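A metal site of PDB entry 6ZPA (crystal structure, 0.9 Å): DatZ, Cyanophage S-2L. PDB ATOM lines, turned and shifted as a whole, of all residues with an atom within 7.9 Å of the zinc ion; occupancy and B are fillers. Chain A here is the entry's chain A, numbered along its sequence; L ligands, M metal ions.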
ATOM      1  N   ARG A  25      33.976  -8.131  14.899  1.00  0.00           N
ATOM      2  CA  ARG A  25      33.496  -7.794  13.570  1.00  0.00           C
ATOM      3  C   ARG A  25      34.604  -7.112  12.761  1.00  0.00           C
ATOM      4  O   ARG A  25      35.696  -6.832  13.257  1.00  0.00           O
ATOM      5  CB  ARG A  25      32.253  -6.907  13.690  1.00  0.00           C
ATOM      6  CG  ARG A  25      31.045  -7.693  14.156  1.00  0.00           C
ATOM      7  CD  ARG A  25      29.895  -6.793  14.571  1.00  0.00           C
ATOM      8  NE  ARG A  25      29.503  -5.811  13.545  1.00  0.00           N
ATOM      9  CZ  ARG A  25      28.709  -6.049  12.504  1.00  0.00           C
ATOM     10  NH1 ARG A  25      28.203  -7.256  12.301  1.00  0.00           N
ATOM     11  NH2 ARG A  25      28.420  -5.065  11.670  1.00  0.00           N
ATOM     12  N   ILE A  37      30.226  -8.505  18.679  1.00  0.00           N
ATOM     13  CA  ILE A  37      28.869  -8.752  18.215  1.00  0.00           C
ATOM     14  C   ILE A  37      27.822  -8.406  19.277  1.00  0.00           C
ATOM     15  O   ILE A  37      26.659  -8.202  18.924  1.00  0.00           O
ATOM     16  CB  ILE A  37      28.636 -10.157  17.626  1.00  0.00           C
ATOM     17  CG1 ILE A  37      28.614 -11.251  18.700  1.00  0.00           C
ATOM     18  CG2 ILE A  37      29.644 -10.436  16.513  1.00  0.00           C
ATOM     19  CD1 ILE A  37      28.226 -12.608  18.166  1.00  0.00           C
ATOM     20  N   HIS A  40      27.164  -4.749  18.730  1.00  0.00           N
ATOM     21  CA  HIS A  40      26.436  -4.694  17.456  1.00  0.00           C
ATOM     22  C   HIS A  40      24.977  -5.087  17.644  1.00  0.00           C
ATOM     23  O   HIS A  40      24.077  -4.385  17.176  1.00  0.00           O
ATOM     24  CB  HIS A  40      27.142  -5.583  16.428  1.00  0.00           C
ATOM     25  CG  HIS A  40      26.309  -5.961  15.241  1.00  0.00           C
ATOM     26  ND1 HIS A  40      25.984  -5.096  14.219  1.00  0.00           N
ATOM     27  CD2 HIS A  40      25.764  -7.159  14.895  1.00  0.00           C
ATOM     28  CE1 HIS A  40      25.257  -5.751  13.314  1.00  0.00           C
ATOM     29  NE2 HIS A  40      25.109  -6.994  13.697  1.00  0.00           N
ATOM     30  N   MET A  41      24.717  -6.225  18.291  1.00  0.00           N
ATOM     31  CA  MET A  41      23.342  -6.690  18.422  1.00  0.00           C
ATOM     32  C   MET A  41      22.517  -5.728  19.268  1.00  0.00           C
ATOM     33  O   MET A  41      21.337  -5.492  18.968  1.00  0.00           O
ATOM     34  CB  MET A  41      23.282  -8.111  18.959  1.00  0.00           C
ATOM     35  CG  MET A  41      23.708  -9.133  17.900  1.00  0.00           C
ATOM     36  SD  MET A  41      23.403 -10.860  18.332  1.00  0.00           S
ATOM     37  CE  MET A  41      24.689 -11.132  19.537  1.00  0.00           C
ATOM     38  N   VAL A  44      21.678  -2.834  16.931  1.00  0.00           N
ATOM     39  CA  VAL A  44      20.665  -3.214  15.948  1.00  0.00           C
ATOM     40  C   VAL A  44      19.291  -3.308  16.599  1.00  0.00           C
ATOM     41  O   VAL A  44      18.284  -2.859  16.035  1.00  0.00           O
ATOM     42  CB  VAL A  44      21.047  -4.532  15.232  1.00  0.00           C
ATOM     43  CG1 VAL A  44      19.940  -4.985  14.293  1.00  0.00           C
ATOM     44  CG2 VAL A  44      22.342  -4.355  14.442  1.00  0.00           C
ATOM     45  N   PHE A  68      14.725 -10.888  17.230  1.00  0.00           N
ATOM     46  CA  PHE A  68      15.739 -11.471  16.376  1.00  0.00           C
ATOM     47  C   PHE A  68      17.037 -10.682  16.461  1.00  0.00           C
ATOM     48  O   PHE A  68      18.123 -11.266  16.503  1.00  0.00           O
ATOM     49  CB  PHE A  68      15.242 -11.523  14.928  1.00  0.00           C
ATOM     50  CG  PHE A  68      16.151 -12.282  14.000  1.00  0.00           C
ATOM     51  CD1 PHE A  68      16.431 -13.625  14.211  1.00  0.00           C
ATOM     52  CD2 PHE A  68      16.708 -11.661  12.879  1.00  0.00           C
ATOM     53  CE1 PHE A  68      17.264 -14.324  13.340  1.00  0.00           C
ATOM     54  CE2 PHE A  68      17.535 -12.356  12.015  1.00  0.00           C
ATOM     55  CZ  PHE A  68      17.796 -13.694  12.236  1.00  0.00           C
ATOM     56  N   ALA A  69      16.947  -9.345  16.523  1.00  0.00           N
ATOM     57  CA  ALA A  69      18.134  -8.512  16.587  1.00  0.00           C
ATOM     58  C   ALA A  69      19.063  -8.944  17.713  1.00  0.00           C
ATOM     59  O   ALA A  69      20.287  -8.927  17.550  1.00  0.00           O
ATOM     60  CB  ALA A  69      17.742  -7.049  16.776  1.00  0.00           C
ATOM     61  N   HIS A  72      20.637 -12.601  16.594  1.00  0.00           N
ATOM     62  CA  HIS A  72      20.738 -13.057  15.210  1.00  0.00           C
ATOM     63  C   HIS A  72      22.147 -13.497  14.821  1.00  0.00           C
ATOM     64  O   HIS A  72      22.286 -14.312  13.908  1.00  0.00           O
ATOM     65  CB  HIS A  72      20.222 -11.972  14.259  1.00  0.00           C
ATOM     66  CG  HIS A  72      21.122 -10.779  14.126  1.00  0.00           C
ATOM     67  ND1 HIS A  72      21.133  -9.724  15.017  1.00  0.00           N
ATOM     68  CD2 HIS A  72      22.011 -10.453  13.165  1.00  0.00           C
ATOM     69  CE1 HIS A  72      22.003  -8.809  14.603  1.00  0.00           C
ATOM     70  NE2 HIS A  72      22.553  -9.231  13.477  1.00  0.00           N
ATOM     71  N   ASP A  73      23.185 -12.962  15.467  1.00  0.00           N
ATOM     72  CA  ASP A  73      24.565 -13.293  15.127  1.00  0.00           C
ATOM     73  C   ASP A  73      25.195 -14.283  16.110  1.00  0.00           C
ATOM     74  O   ASP A  73      26.409 -14.496  16.052  1.00  0.00           O
ATOM     75  CB  ASP A  73      25.411 -12.026  14.971  1.00  0.00           C
ATOM     76  CG  ASP A  73      25.152 -11.306  13.643  1.00  0.00           C
ATOM     77  OD1 ASP A  73      24.751 -11.986  12.665  1.00  0.00           O
ATOM     78  OD2 ASP A  73      25.349 -10.072  13.577  1.00  0.00           O
ATOM     79  N   GLU A  76      27.999 -16.862  15.297  1.00  0.00           N
ATOM     80  CA  GLU A  76      29.364 -16.405  15.073  1.00  0.00           C
ATOM     81  C   GLU A  76      30.271 -16.706  16.254  1.00  0.00           C
ATOM     82  O   GLU A  76      31.490 -16.667  16.101  1.00  0.00           O
ATOM     83  CB  GLU A  76      29.363 -14.913  14.733  1.00  0.00           C
ATOM     84  CG  GLU A  76      28.649 -14.617  13.424  1.00  0.00           C
ATOM     85  CD  GLU A  76      28.622 -13.152  13.064  1.00  0.00           C
ATOM     86  OE1 GLU A  76      28.953 -12.322  13.925  1.00  0.00           O
ATOM     87  OE2 GLU A  76      28.270 -12.821  11.910  1.00  0.00           O
ATOM     88  N   ASP A  81      32.703 -14.064  12.474  1.00  0.00           N
ATOM     89  CA  ASP A  81      32.009 -13.127  11.620  1.00  0.00           C
ATOM     90  C   ASP A  81      32.789 -13.056  10.310  1.00  0.00           C
ATOM     91  O   ASP A  81      34.013 -12.859  10.321  1.00  0.00           O
ATOM     92  CB  ASP A  81      31.956 -11.772  12.311  1.00  0.00           C
ATOM     93  CG  ASP A  81      31.575 -10.654  11.379  1.00  0.00           C
ATOM     94  OD1 ASP A  81      30.376 -10.569  11.032  1.00  0.00           O
ATOM     95  OD2 ASP A  81      32.471  -9.893  10.974  1.00  0.00           O
ATOM     96  N   LYS A  87      30.202 -13.777   1.527  1.00  0.00           N
ATOM     97  CA  LYS A  87      29.031 -14.624   1.740  1.00  0.00           C
ATOM     98  C   LYS A  87      28.221 -14.719   0.453  1.00  0.00           C
ATOM     99  O   LYS A  87      27.159 -14.102   0.290  1.00  0.00           O
ATOM    100  CB  LYS A  87      28.178 -14.084   2.881  1.00  0.00           C
ATOM    101  CG  LYS A  87      28.861 -14.058   4.225  1.00  0.00           C
ATOM    102  CD  LYS A  87      27.903 -13.505   5.251  1.00  0.00           C
ATOM    103  CE  LYS A  87      28.523 -13.403   6.622  1.00  0.00           C
ATOM    104  NZ  LYS A  87      27.605 -12.737   7.575  1.00  0.00           N
ATOM    105  N   TRP A 121      14.658  -5.490  10.285  1.00  0.00           N
ATOM    106  CA  TRP A 121      15.901  -5.965  10.878  1.00  0.00           C
ATOM    107  C   TRP A 121      17.074  -5.787   9.906  1.00  0.00           C
ATOM    108  O   TRP A 121      18.140  -5.311  10.289  1.00  0.00           O
ATOM    109  CB  TRP A 121      15.771  -7.426  11.337  1.00  0.00           C
ATOM    110  CG  TRP A 121      17.117  -8.045  11.493  1.00  0.00           C
ATOM    111  CD1 TRP A 121      18.021  -7.834  12.499  1.00  0.00           C
ATOM    112  CD2 TRP A 121      17.762  -8.890  10.546  1.00  0.00           C
ATOM    113  NE1 TRP A 121      19.192  -8.514  12.233  1.00  0.00           N
ATOM    114  CE2 TRP A 121      19.049  -9.172  11.044  1.00  0.00           C
ATOM    115  CE3 TRP A 121      17.375  -9.433   9.321  1.00  0.00           C
ATOM    116  CZ2 TRP A 121      19.933  -9.999  10.365  1.00  0.00           C
ATOM    117  CZ3 TRP A 121      18.253 -10.238   8.651  1.00  0.00           C
ATOM    118  CH2 TRP A 121      19.517 -10.518   9.173  1.00  0.00           C
ATOM    119  N   LYS A 122      16.892  -6.171   8.630  1.00  0.00           N
ATOM    120  CA  LYS A 122      18.019  -6.102   7.709  1.00  0.00           C
ATOM    121  C   LYS A 122      18.450  -4.665   7.466  1.00  0.00           C
ATOM    122  O   LYS A 122      19.651  -4.364   7.386  1.00  0.00           O
ATOM    123  CB  LYS A 122      17.669  -6.799   6.399  1.00  0.00           C
ATOM    124  CG  LYS A 122      18.842  -6.862   5.429  1.00  0.00           C
ATOM    125  CD  LYS A 122      20.066  -7.512   6.052  1.00  0.00           C
ATOM    126  CE  LYS A 122      21.221  -7.527   5.078  1.00  0.00           C
ATOM    127  NZ  LYS A 122      22.307  -8.462   5.509  1.00  0.00           N
ATOM    128  N   CYS A 124      18.188  -2.216   9.576  1.00  0.00           N
ATOM    129  CA  CYS A 124      18.854  -1.756  10.786  1.00  0.00           C
ATOM    130  C   CYS A 124      20.223  -2.420  10.962  1.00  0.00           C
ATOM    131  O   CYS A 124      21.156  -1.778  11.459  1.00  0.00           O
ATOM    132  CB  CYS A 124      17.973  -2.034  12.002  1.00  0.00           C
ATOM    133  SG  CYS A 124      16.487  -0.978  12.021  1.00  0.00           S
ATOM    134  N   ASP A 125      20.349  -3.689  10.588  1.00  0.00           N
ATOM    135  CA  ASP A 125      21.625  -4.391  10.681  1.00  0.00           C
ATOM    136  C   ASP A 125      22.680  -3.711   9.813  1.00  0.00           C
ATOM    137  O   ASP A 125      23.831  -3.511  10.236  1.00  0.00           O
ATOM    138  CB  ASP A 125      21.417  -5.848  10.252  1.00  0.00           C
ATOM    139  CG  ASP A 125      22.644  -6.694  10.462  1.00  0.00           C
ATOM    140  OD1 ASP A 125      22.993  -6.950  11.622  1.00  0.00           O
ATOM    141  OD2 ASP A 125      23.273  -7.087   9.473  1.00  0.00           O
ATOM    142  N   THR A 126      22.300  -3.339   8.592  1.00  0.00           N
ATOM    143  CA  THR A 126      23.225  -2.662   7.704  1.00  0.00           C
ATOM    144  C   THR A 126      23.451  -1.219   8.143  1.00  0.00           C
ATOM    145  O   THR A 126      24.589  -0.729   8.117  1.00  0.00           O
ATOM    146  CB  THR A 126      22.715  -2.732   6.257  1.00  0.00           C
ATOM    147  OG1 THR A 126      22.459  -4.093   5.914  1.00  0.00           O
ATOM    148  CG2 THR A 126      23.735  -2.153   5.295  1.00  0.00           C
ATOM    149  N   GLU A 128      23.419  -0.018  11.113  1.00  0.00           N
ATOM    150  CA  GLU A 128      24.315  -0.009  12.266  1.00  0.00           C
ATOM    151  C   GLU A 128      25.767  -0.067  11.816  1.00  0.00           C
ATOM    152  O   GLU A 128      26.633   0.606  12.397  1.00  0.00           O
ATOM    153  CB  GLU A 128      23.975  -1.159  13.208  1.00  0.00           C
ATOM    154  CG  GLU A 128      24.699  -1.097  14.548  1.00  0.00           C
ATOM    155  CD  GLU A 128      26.169  -1.520  14.497  1.00  0.00           C
ATOM    156  OE1 GLU A 128      26.982  -0.951  15.268  1.00  0.00           O
ATOM    157  OE2 GLU A 128      26.487  -2.444  13.709  1.00  0.00           O
ATOM    158  N   ALA A 129      26.036  -0.879  10.790  1.00  0.00           N
ATOM    159  CA  ALA A 129      27.396  -1.027  10.277  1.00  0.00           C
ATOM    160  C   ALA A 129      27.886   0.261   9.622  1.00  0.00           C
ATOM    161  O   ALA A 129      29.033   0.680   9.831  1.00  0.00           O
ATOM    162  CB  ALA A 129      27.416  -2.199   9.284  1.00  0.00           C
HETATM  163  O1  LIG L   1      28.206  -8.940   9.177  1.00  0.00           O
HETATM  164  C1  LIG L   1      29.051  -8.885   8.022  1.00  0.00           C
HETATM  165  C2  LIG L   1      30.471  -8.526   8.389  1.00  0.00           C
HETATM  166  O2  LIG L   1      31.155  -8.007   7.223  1.00  0.00           O
HETATM  167  C3  LIG L   1      31.498  -6.656   7.424  1.00  0.00           C
HETATM  168  N1  LIG L   1      31.315  -5.986   6.152  1.00  0.00           N
HETATM  169  C4  LIG L   1      32.299  -5.844   5.206  1.00  0.00           C
HETATM  170  N2  LIG L   1      33.602  -6.106   5.334  1.00  0.00           N
HETATM  171  C5  LIG L   1      34.259  -5.863   4.200  1.00  0.00           C
HETATM  172  N3  LIG L   1      33.771  -5.419   3.030  1.00  0.00           N
HETATM  173  C6  LIG L   1      32.461  -5.144   2.932  1.00  0.00           C
HETATM  174  N4  LIG L   1      31.981  -4.678   1.768  1.00  0.00           N
HETATM  175  C7  LIG L   1      31.657  -5.360   4.069  1.00  0.00           C
HETATM  176  N5  LIG L   1      30.310  -5.170   4.311  1.00  0.00           N
HETATM  177  C8  LIG L   1      30.155  -5.557   5.558  1.00  0.00           C
HETATM  178  C9  LIG L   1      30.644  -6.177   8.576  1.00  0.00           C
HETATM  179  C10 LIG L   1      30.581  -7.428   9.440  1.00  0.00           C
HETATM  180  O3  LIG L   1      31.793  -7.520  10.190  1.00  0.00           O
HETATM  181 ZN    ZN M   1      24.242  -8.484  12.367  1.00  0.00          ZN
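The backbone NH of Asp 73 is in hydrogen-bond range of the side-chain sulfur of Met 41, at 3.6 Å. A ring nitrogen (NE2) of His 40 sits close to the guanidinium group (NH1) of Arg 25, at 3.4 Å. ND1 of His 40 sits at hydrogen-bond distance from OE2 of Glu 128, 2.7 Å away. ND1 of His 72 sits at hydrogen-bond distance from O of Ala 69 (2.8 Å). SD of Met 41 is in hydrogen-bond range of N of His 72, at 3.7 Å.
The zinc ion is bound by OD1 of Asp 125 (2.1 Å), NE2 of His 72 (2.2 Å), NE2 of His 40 (2.2 Å) and OD2 of Asp 73 (2.3 Å).
Of the 19 residues printed, 4 come within 4 Å of the zinc ion. The nearest printed residue that does not touch the zinc ion is Arg 25 (4.1 Å).
The side-chain carboxylate of Asp 81 lies within hydrogen-bond range of an oxygen (O3) of the ligand, at 2.6 Å.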
